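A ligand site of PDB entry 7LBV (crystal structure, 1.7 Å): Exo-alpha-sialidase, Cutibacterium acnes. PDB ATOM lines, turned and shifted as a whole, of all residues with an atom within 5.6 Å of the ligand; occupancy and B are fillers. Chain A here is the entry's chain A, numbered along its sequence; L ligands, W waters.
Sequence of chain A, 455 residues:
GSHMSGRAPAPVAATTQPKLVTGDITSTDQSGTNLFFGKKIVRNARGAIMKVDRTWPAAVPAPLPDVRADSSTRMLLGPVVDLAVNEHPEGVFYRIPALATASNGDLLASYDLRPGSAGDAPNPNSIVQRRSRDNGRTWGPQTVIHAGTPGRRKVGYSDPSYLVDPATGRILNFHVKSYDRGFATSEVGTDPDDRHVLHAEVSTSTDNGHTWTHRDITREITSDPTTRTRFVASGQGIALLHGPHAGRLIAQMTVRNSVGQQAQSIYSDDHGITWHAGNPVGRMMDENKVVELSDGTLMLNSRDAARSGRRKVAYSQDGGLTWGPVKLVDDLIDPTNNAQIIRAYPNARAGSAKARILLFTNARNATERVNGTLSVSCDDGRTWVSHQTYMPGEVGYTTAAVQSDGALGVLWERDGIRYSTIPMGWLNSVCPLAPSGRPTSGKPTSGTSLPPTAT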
ATOM      1  N   ARG A  95      25.754 -30.321   9.996  1.00  0.00           N
ATOM      2  CA  ARG A  95      24.508 -29.589  10.287  1.00  0.00           C
ATOM      3  C   ARG A  95      24.882 -28.174  10.723  1.00  0.00           C
ATOM      4  O   ARG A  95      26.035 -27.927  11.122  1.00  0.00           O
ATOM      5  CB  ARG A  95      23.750 -30.228  11.478  1.00  0.00           C
ATOM      6  CG  ARG A  95      22.842 -31.402  10.978  1.00  0.00           C
ATOM      7  CD  ARG A  95      21.633 -31.526  11.932  1.00  0.00           C
ATOM      8  NE  ARG A  95      20.767 -30.313  11.802  1.00  0.00           N
ATOM      9  CZ  ARG A  95      19.828 -29.908  12.665  1.00  0.00           C
ATOM     10  NH1 ARG A  95      19.590 -30.607  13.796  1.00  0.00           N
ATOM     11  NH2 ARG A  95      19.151 -28.781  12.419  1.00  0.00           N
ATOM     12  N   ILE A  96      23.907 -27.268  10.660  1.00  0.00           N
ATOM     13  CA  ILE A  96      23.894 -25.951  11.357  1.00  0.00           C
ATOM     14  C   ILE A  96      24.725 -24.864  10.592  1.00  0.00           C
ATOM     15  O   ILE A  96      25.886 -24.546  10.967  1.00  0.00           O
ATOM     16  CB  ILE A  96      24.298 -25.972  12.829  1.00  0.00           C
ATOM     17  CG1 ILE A  96      23.801 -27.242  13.583  1.00  0.00           C
ATOM     18  CG2 ILE A  96      23.781 -24.698  13.486  1.00  0.00           C
ATOM     19  CD1 ILE A  96      22.265 -27.517  13.596  1.00  0.00           C
ATOM     20  N   ASP A 112      28.671 -27.296  11.638  1.00  0.00           N
ATOM     21  CA  ASP A 112      29.178 -28.347  12.555  1.00  0.00           C
ATOM     22  C   ASP A 112      29.684 -29.561  11.742  1.00  0.00           C
ATOM     23  O   ASP A 112      29.024 -29.994  10.793  1.00  0.00           O
ATOM     24  CB  ASP A 112      28.063 -28.916  13.441  1.00  0.00           C
ATOM     25  CG  ASP A 112      27.693 -28.035  14.643  1.00  0.00           C
ATOM     26  OD1 ASP A 112      28.056 -26.838  14.706  1.00  0.00           O
ATOM     27  OD2 ASP A 112      27.008 -28.584  15.522  1.00  0.00           O
ATOM     28  N   ARG A 114      29.775 -33.244  12.967  1.00  0.00           N
ATOM     29  CA  ARG A 114      29.204 -33.981  14.073  1.00  0.00           C
ATOM     30  C   ARG A 114      29.626 -35.455  13.948  1.00  0.00           C
ATOM     31  O   ARG A 114      29.203 -36.140  13.006  1.00  0.00           O
ATOM     32  CB  ARG A 114      27.672 -33.878  14.026  1.00  0.00           C
ATOM     33  CG  ARG A 114      27.258 -32.389  14.184  1.00  0.00           C
ATOM     34  CD  ARG A 114      25.773 -32.273  14.322  1.00  0.00           C
ATOM     35  NE  ARG A 114      25.485 -30.955  14.886  1.00  0.00           N
ATOM     36  CZ  ARG A 114      24.364 -30.616  15.531  1.00  0.00           C
ATOM     37  NH1 ARG A 114      23.305 -31.472  15.565  1.00  0.00           N
ATOM     38  NH2 ARG A 114      24.281 -29.355  16.030  1.00  0.00           N
ATOM     39  N   ASP A 120      23.210 -33.028  18.664  1.00  0.00           N
ATOM     40  CA  ASP A 120      23.485 -31.694  19.129  1.00  0.00           C
ATOM     41  C   ASP A 120      24.514 -31.781  20.266  1.00  0.00           C
ATOM     42  O   ASP A 120      24.821 -32.897  20.766  1.00  0.00           O
ATOM     43  CB  ASP A 120      22.205 -31.144  19.741  1.00  0.00           C
ATOM     44  CG  ASP A 120      21.040 -30.988  18.711  1.00  0.00           C
ATOM     45  OD1 ASP A 120      21.265 -30.751  17.541  1.00  0.00           O
ATOM     46  OD2 ASP A 120      19.899 -30.971  19.138  1.00  0.00           O
ATOM     47  N   ALA A 121      25.031 -30.641  20.710  1.00  0.00           N
ATOM     48  CA  ALA A 121      25.722 -30.624  22.049  1.00  0.00           C
ATOM     49  C   ALA A 121      24.933 -31.435  23.104  1.00  0.00           C
ATOM     50  O   ALA A 121      23.714 -31.368  23.180  1.00  0.00           O
ATOM     51  CB  ALA A 121      25.966 -29.183  22.560  1.00  0.00           C
ATOM     52  N   SER A 158      29.937 -26.225  18.777  1.00  0.00           N
ATOM     53  CA  SER A 158      28.704 -26.512  17.978  1.00  0.00           C
ATOM     54  C   SER A 158      27.821 -25.240  17.795  1.00  0.00           C
ATOM     55  O   SER A 158      27.748 -24.384  18.687  1.00  0.00           O
ATOM     56  CB  SER A 158      27.957 -27.647  18.731  1.00  0.00           C
ATOM     57  OG  SER A 158      26.866 -28.211  17.961  1.00  0.00           O
ATOM     58  N   ASP A 159      27.151 -25.146  16.629  1.00  0.00           N
ATOM     59  CA  ASP A 159      26.146 -24.101  16.289  1.00  0.00           C
ATOM     60  C   ASP A 159      26.899 -22.783  16.053  1.00  0.00           C
ATOM     61  O   ASP A 159      26.884 -21.887  16.930  1.00  0.00           O
ATOM     62  CB  ASP A 159      25.080 -23.889  17.407  1.00  0.00           C
ATOM     63  CG  ASP A 159      23.955 -24.866  17.357  1.00  0.00           C
ATOM     64  OD1 ASP A 159      24.184 -26.033  17.015  1.00  0.00           O
ATOM     65  OD2 ASP A 159      22.861 -24.493  17.791  1.00  0.00           O
ATOM     66  N   VAL A 176      28.665 -22.756  20.799  1.00  0.00           N
ATOM     67  CA  VAL A 176      28.776 -23.308  22.157  1.00  0.00           C
ATOM     68  C   VAL A 176      30.141 -23.970  22.358  1.00  0.00           C
ATOM     69  O   VAL A 176      30.841 -24.335  21.416  1.00  0.00           O
ATOM     70  CB  VAL A 176      27.629 -24.283  22.547  1.00  0.00           C
ATOM     71  CG1 VAL A 176      26.231 -23.749  22.162  1.00  0.00           C
ATOM     72  CG2 VAL A 176      27.907 -25.650  21.918  1.00  0.00           C
ATOM     73  N   PHE A 183      22.163 -27.821  25.785  1.00  0.00           N
ATOM     74  CA  PHE A 183      21.286 -26.666  26.083  1.00  0.00           C
ATOM     75  C   PHE A 183      20.261 -26.990  27.195  1.00  0.00           C
ATOM     76  O   PHE A 183      20.129 -26.251  28.176  1.00  0.00           O
ATOM     77  CB  PHE A 183      20.534 -26.201  24.853  1.00  0.00           C
ATOM     78  CG  PHE A 183      19.502 -25.122  25.124  1.00  0.00           C
ATOM     79  CD1 PHE A 183      19.892 -23.777  25.456  1.00  0.00           C
ATOM     80  CD2 PHE A 183      18.118 -25.402  24.963  1.00  0.00           C
ATOM     81  CE1 PHE A 183      18.912 -22.795  25.683  1.00  0.00           C
ATOM     82  CE2 PHE A 183      17.158 -24.388  25.139  1.00  0.00           C
ATOM     83  CZ  PHE A 183      17.550 -23.120  25.558  1.00  0.00           C
ATOM     84  N   LEU A 198      26.880 -25.361  29.907  1.00  0.00           N
ATOM     85  CA  LEU A 198      27.053 -25.105  28.464  1.00  0.00           C
ATOM     86  C   LEU A 198      27.681 -23.759  28.293  1.00  0.00           C
ATOM     87  O   LEU A 198      27.030 -22.772  28.628  1.00  0.00           O
ATOM     88  CB  LEU A 198      25.718 -25.164  27.692  1.00  0.00           C
ATOM     89  CG  LEU A 198      25.848 -25.029  26.132  1.00  0.00           C
ATOM     90  CD1 LEU A 198      26.657 -26.129  25.501  1.00  0.00           C
ATOM     91  CD2 LEU A 198      24.499 -25.039  25.437  1.00  0.00           C
ATOM     92  N   PHE A 231      22.745 -20.205  24.282  1.00  0.00           N
ATOM     93  CA  PHE A 231      23.477 -20.400  23.049  1.00  0.00           C
ATOM     94  C   PHE A 231      23.172 -19.241  22.088  1.00  0.00           C
ATOM     95  O   PHE A 231      22.015 -18.834  21.973  1.00  0.00           O
ATOM     96  CB  PHE A 231      23.267 -21.814  22.434  1.00  0.00           C
ATOM     97  CG  PHE A 231      21.901 -22.076  21.825  1.00  0.00           C
ATOM     98  CD1 PHE A 231      20.744 -22.232  22.599  1.00  0.00           C
ATOM     99  CD2 PHE A 231      21.793 -22.334  20.424  1.00  0.00           C
ATOM    100  CE1 PHE A 231      19.493 -22.528  22.036  1.00  0.00           C
ATOM    101  CE2 PHE A 231      20.556 -22.677  19.856  1.00  0.00           C
ATOM    102  CZ  PHE A 231      19.394 -22.725  20.656  1.00  0.00           C
ATOM    103  N   ARG A 256      17.798 -19.854  29.335  1.00  0.00           N
ATOM    104  CA  ARG A 256      16.778 -20.209  30.311  1.00  0.00           C
ATOM    105  C   ARG A 256      17.200 -19.623  31.639  1.00  0.00           C
ATOM    106  O   ARG A 256      18.389 -19.769  32.034  1.00  0.00           O
ATOM    107  CB  ARG A 256      16.616 -21.753  30.482  1.00  0.00           C
ATOM    108  CG  ARG A 256      16.011 -22.427  29.285  1.00  0.00           C
ATOM    109  CD  ARG A 256      15.975 -23.932  29.493  1.00  0.00           C
ATOM    110  NE  ARG A 256      15.346 -24.518  28.307  1.00  0.00           N
ATOM    111  CZ  ARG A 256      15.116 -25.829  28.135  1.00  0.00           C
ATOM    112  NH1 ARG A 256      15.491 -26.721  29.055  1.00  0.00           N
ATOM    113  NH2 ARG A 256      14.511 -26.237  26.999  1.00  0.00           N
ATOM    114  N   GLN A 261      12.273 -19.247  29.145  1.00  0.00           N
ATOM    115  CA  GLN A 261      13.156 -19.402  27.986  1.00  0.00           C
ATOM    116  C   GLN A 261      13.018 -18.128  27.177  1.00  0.00           C
ATOM    117  O   GLN A 261      12.025 -17.944  26.443  1.00  0.00           O
ATOM    118  CB  GLN A 261      12.804 -20.652  27.180  1.00  0.00           C
ATOM    119  CG  GLN A 261      13.841 -20.878  26.020  1.00  0.00           C
ATOM    120  CD  GLN A 261      13.783 -22.307  25.500  1.00  0.00           C
ATOM    121  OE1 GLN A 261      13.850 -23.271  26.270  1.00  0.00           O
ATOM    122  NE2 GLN A 261      13.658 -22.461  24.200  1.00  0.00           N
ATOM    123  N   ASP A 286      13.352 -18.811  21.218  1.00  0.00           N
ATOM    124  CA  ASP A 286      14.341 -19.801  20.816  1.00  0.00           C
ATOM    125  C   ASP A 286      15.259 -19.061  19.851  1.00  0.00           C
ATOM    126  O   ASP A 286      15.317 -17.823  19.868  1.00  0.00           O
ATOM    127  CB  ASP A 286      13.693 -21.060  20.193  1.00  0.00           C
ATOM    128  CG  ASP A 286      14.528 -22.288  20.396  1.00  0.00           C
ATOM    129  OD1 ASP A 286      15.726 -22.289  19.970  1.00  0.00           O
ATOM    130  OD2 ASP A 286      14.021 -23.208  21.073  1.00  0.00           O
ATOM    131  N   GLU A 287      16.003 -19.793  19.023  1.00  0.00           N
ATOM    132  CA  GLU A 287      16.935 -19.114  18.097  1.00  0.00           C
ATOM    133  C   GLU A 287      16.278 -17.901  17.447  1.00  0.00           C
ATOM    134  O   GLU A 287      15.152 -17.991  16.905  1.00  0.00           O
ATOM    135  CB  GLU A 287      17.308 -20.081  16.968  1.00  0.00           C
ATOM    136  CG  GLU A 287      18.178 -21.248  17.433  1.00  0.00           C
ATOM    137  CD  GLU A 287      18.027 -22.490  16.579  1.00  0.00           C
ATOM    138  OE1 GLU A 287      16.989 -22.616  15.900  1.00  0.00           O
ATOM    139  OE2 GLU A 287      18.960 -23.316  16.629  1.00  0.00           O
ATOM    140  N   ARG A 303      12.369 -17.971  16.353  1.00  0.00           N
ATOM    141  CA  ARG A 303      11.705 -19.269  16.375  1.00  0.00           C
ATOM    142  C   ARG A 303      10.819 -19.337  17.636  1.00  0.00           C
ATOM    143  O   ARG A 303      11.179 -18.726  18.663  1.00  0.00           O
ATOM    144  CB  ARG A 303      12.820 -20.319  16.396  1.00  0.00           C
ATOM    145  CG  ARG A 303      12.424 -21.774  16.742  1.00  0.00           C
ATOM    146  CD  ARG A 303      13.707 -22.610  16.788  1.00  0.00           C
ATOM    147  NE  ARG A 303      13.482 -23.993  17.347  1.00  0.00           N
ATOM    148  CZ  ARG A 303      14.268 -25.047  17.072  1.00  0.00           C
ATOM    149  NH1 ARG A 303      15.334 -24.946  16.278  1.00  0.00           N
ATOM    150  NH2 ARG A 303      13.996 -26.209  17.676  1.00  0.00           N
ATOM    151  N   THR A 336       8.853 -24.154  13.739  1.00  0.00           N
ATOM    152  CA  THR A 336       9.713 -24.090  14.975  1.00  0.00           C
ATOM    153  C   THR A 336      11.103 -24.597  14.569  1.00  0.00           C
ATOM    154  O   THR A 336      11.470 -25.774  14.765  1.00  0.00           O
ATOM    155  CB  THR A 336       9.060 -24.778  16.201  1.00  0.00           C
ATOM    156  OG1 THR A 336       7.901 -24.004  16.470  1.00  0.00           O
ATOM    157  CG2 THR A 336      10.017 -24.756  17.422  1.00  0.00           C
ATOM    158  N   ASN A 337      11.834 -23.714  13.880  1.00  0.00           N
ATOM    159  CA  ASN A 337      13.064 -24.100  13.153  1.00  0.00           C
ATOM    160  C   ASN A 337      13.884 -22.838  13.046  1.00  0.00           C
ATOM    161  O   ASN A 337      13.349 -21.741  13.181  1.00  0.00           O
ATOM    162  CB  ASN A 337      12.611 -24.624  11.788  1.00  0.00           C
ATOM    163  CG  ASN A 337      13.715 -25.160  10.913  1.00  0.00           C
ATOM    164  OD1 ASN A 337      14.739 -25.752  11.399  1.00  0.00           O
ATOM    165  ND2 ASN A 337      13.558 -24.918   9.573  1.00  0.00           N
ATOM    166  N   ARG A 369      10.126 -29.268   8.281  1.00  0.00           N
ATOM    167  CA  ARG A 369      11.179 -28.361   7.866  1.00  0.00           C
ATOM    168  C   ARG A 369      11.474 -28.469   6.370  1.00  0.00           C
ATOM    169  O   ARG A 369      12.587 -28.899   5.968  1.00  0.00           O
ATOM    170  CB  ARG A 369      12.462 -28.516   8.692  1.00  0.00           C
ATOM    171  CG  ARG A 369      12.198 -28.338  10.154  1.00  0.00           C
ATOM    172  CD  ARG A 369      13.390 -28.725  11.006  1.00  0.00           C
ATOM    173  NE  ARG A 369      13.157 -28.278  12.406  1.00  0.00           N
ATOM    174  CZ  ARG A 369      14.152 -28.260  13.315  1.00  0.00           C
ATOM    175  NH1 ARG A 369      15.363 -28.765  13.031  1.00  0.00           N
ATOM    176  NH2 ARG A 369      13.919 -27.802  14.539  1.00  0.00           N
ATOM    177  N   TYR A 397      17.638 -26.227   8.822  1.00  0.00           N
ATOM    178  CA  TYR A 397      18.110 -24.855   8.983  1.00  0.00           C
ATOM    179  C   TYR A 397      18.591 -24.216   7.680  1.00  0.00           C
ATOM    180  O   TYR A 397      19.379 -24.805   6.952  1.00  0.00           O
ATOM    181  CB  TYR A 397      19.322 -24.843   9.980  1.00  0.00           C
ATOM    182  CG  TYR A 397      18.962 -25.067  11.443  1.00  0.00           C
ATOM    183  CD1 TYR A 397      17.723 -25.675  11.879  1.00  0.00           C
ATOM    184  CD2 TYR A 397      19.838 -24.640  12.407  1.00  0.00           C
ATOM    185  CE1 TYR A 397      17.435 -25.831  13.248  1.00  0.00           C
ATOM    186  CE2 TYR A 397      19.572 -24.797  13.765  1.00  0.00           C
ATOM    187  CZ  TYR A 397      18.377 -25.350  14.194  1.00  0.00           C
ATOM    188  OH  TYR A 397      18.075 -25.480  15.491  1.00  0.00           O
HETATM  189  C1  LIG L   1      17.276 -28.362  16.008  1.00  0.00           C
HETATM  190  C2  LIG L   1      18.456 -27.923  16.760  1.00  0.00           C
HETATM  191  C3  LIG L   1      19.763 -27.982  16.405  1.00  0.00           C
HETATM  192  C4  LIG L   1      20.766 -27.073  17.065  1.00  0.00           C
HETATM  193  C5  LIG L   1      20.409 -27.084  18.599  1.00  0.00           C
HETATM  194  C6  LIG L   1      19.000 -26.476  18.702  1.00  0.00           C
HETATM  195  C7  LIG L   1      18.412 -26.255  20.144  1.00  0.00           C
HETATM  196  C8  LIG L   1      16.946 -25.886  20.137  1.00  0.00           C
HETATM  197  C9  LIG L   1      16.521 -25.541  21.599  1.00  0.00           C
HETATM  198  C10 LIG L   1      21.802 -26.549  20.602  1.00  0.00           C
HETATM  199  C11 LIG L   1      22.920 -25.684  21.186  1.00  0.00           C
HETATM  200  N1  LIG L   1      21.381 -26.290  19.364  1.00  0.00           N
HETATM  201  O1  LIG L   1      16.100 -28.063  16.422  1.00  0.00           O
HETATM  202  O2  LIG L   1      17.493 -28.995  14.964  1.00  0.00           O
HETATM  203  O3  LIG L   1      22.000 -27.699  17.129  1.00  0.00           O
HETATM  204  O4  LIG L   1      18.042 -27.330  18.036  1.00  0.00           O
HETATM  205  O5  LIG L   1      18.478 -27.531  20.888  1.00  0.00           O
HETATM  206  O6  LIG L   1      16.790 -24.743  19.258  1.00  0.00           O
HETATM  207  O7  LIG L   1      15.077 -25.517  21.630  1.00  0.00           O
HETATM  208  O8  LIG L   1      21.266 -27.471  21.322  1.00  0.00           O
HETATM  209  O   HOH W   1      24.442 -28.221  19.268  1.00  0.00           O
HETATM  210  O   HOH W   2      13.819 -27.904  20.762  1.00  0.00           O
HETATM  211  O   HOH W   3      22.108 -29.045  23.296  1.00  0.00           O
HETATM  212  O   HOH W   4      13.869 -25.813  24.079  1.00  0.00           O
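Water W3 lies within hydrogen-bond range of O8 of the ligand, N of Phe 183 and O of Ala 121.
Water W4 lies within hydrogen-bond range of an oxygen (O7) of the ligand (2.7 Å), the guanidinium group of Arg 256 (3.0 Å) and the side-chain amide oxygen of Gln 261 (3.4 Å).
Water W1 lies within hydrogen-bond range of the side-chain hydroxyl (OG) of Ser 158, the backbone NH (N) of Ala 121, the side-chain carboxylate (OD1) of Asp 159, an oxygen (O3) of the ligand and the guanidinium group (NH2) of Arg 114.
Ile 96 touches the ligand (CD1 to O3, 3.5 Å).
CG1 of Val 176 touches C11 of the ligand (3.96 Å).
Phe 183 touches the ligand.
Phe 231 touches the ligand (CZ to O6, 3.6 Å).
Glu 287 touches the ligand (OE2 to O6, 3.7 Å).
The nearest printed residue that does not touch the ligand is Gln 261 (4.2 Å).
The backbone NH of Val 176 is in hydrogen-bond range of the backbone carbonyl oxygen of Ser 158 (2.8 Å).
The guanidinium group of Arg 114 is in salt-bridge range of the side-chain carboxylate of Asp 120 (2.9 Å).
The guanidinium group (NH1) of Arg 303 is in salt-bridge range of the side-chain carboxylate (OE1) of Glu 287.
OG of Ser 158 is in hydrogen-bond range of NH2 of Arg 114 (3.4 Å).
The side-chain carboxylate (OD2) of Asp 286 sits at hydrogen-bond distance from the side-chain amide nitrogen (NE2) of Gln 261 (3.2 Å).
The backbone NH of Asp 112 is in hydrogen-bond range of the backbone carbonyl oxygen of Arg 95 (2.8 Å).
The backbone NH of Asp 159 lies within hydrogen-bond range of the side-chain carboxylate of Asp 112, 2.7 Å away.
NE of Arg 369 lies within hydrogen-bond range of OD1 of Asn 337, 3.1 Å away.
NH1 of Arg 369 lies within salt-bridge range of O2 of the ligand, 2.9 Å away.
OD1 of Asp 120 is in hydrogen-bond range of O3 of the ligand (3.2 Å).
O3 of the ligand is in hydrogen-bond range of NH2 of Arg 114 (3.0 Å).
The side-chain hydroxyl (OH) of Tyr 397 sits close to an oxygen (O4) of the ligand, at 3.1 Å.
The side-chain carboxylate of Asp 159 sits at hydrogen-bond distance from an oxygen (O3) of the ligand, at 2.7 Å.
The guanidinium group of Arg 303 lies within salt-bridge range of an oxygen (O1) of the ligand, 3.1 Å away.
The guanidinium group of Arg 95 is in salt-bridge range of an oxygen (O2) of the ligand (2.9 Å).
O7 of the ligand is in hydrogen-bond range of OD2 of Asp 286 (2.6 Å).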
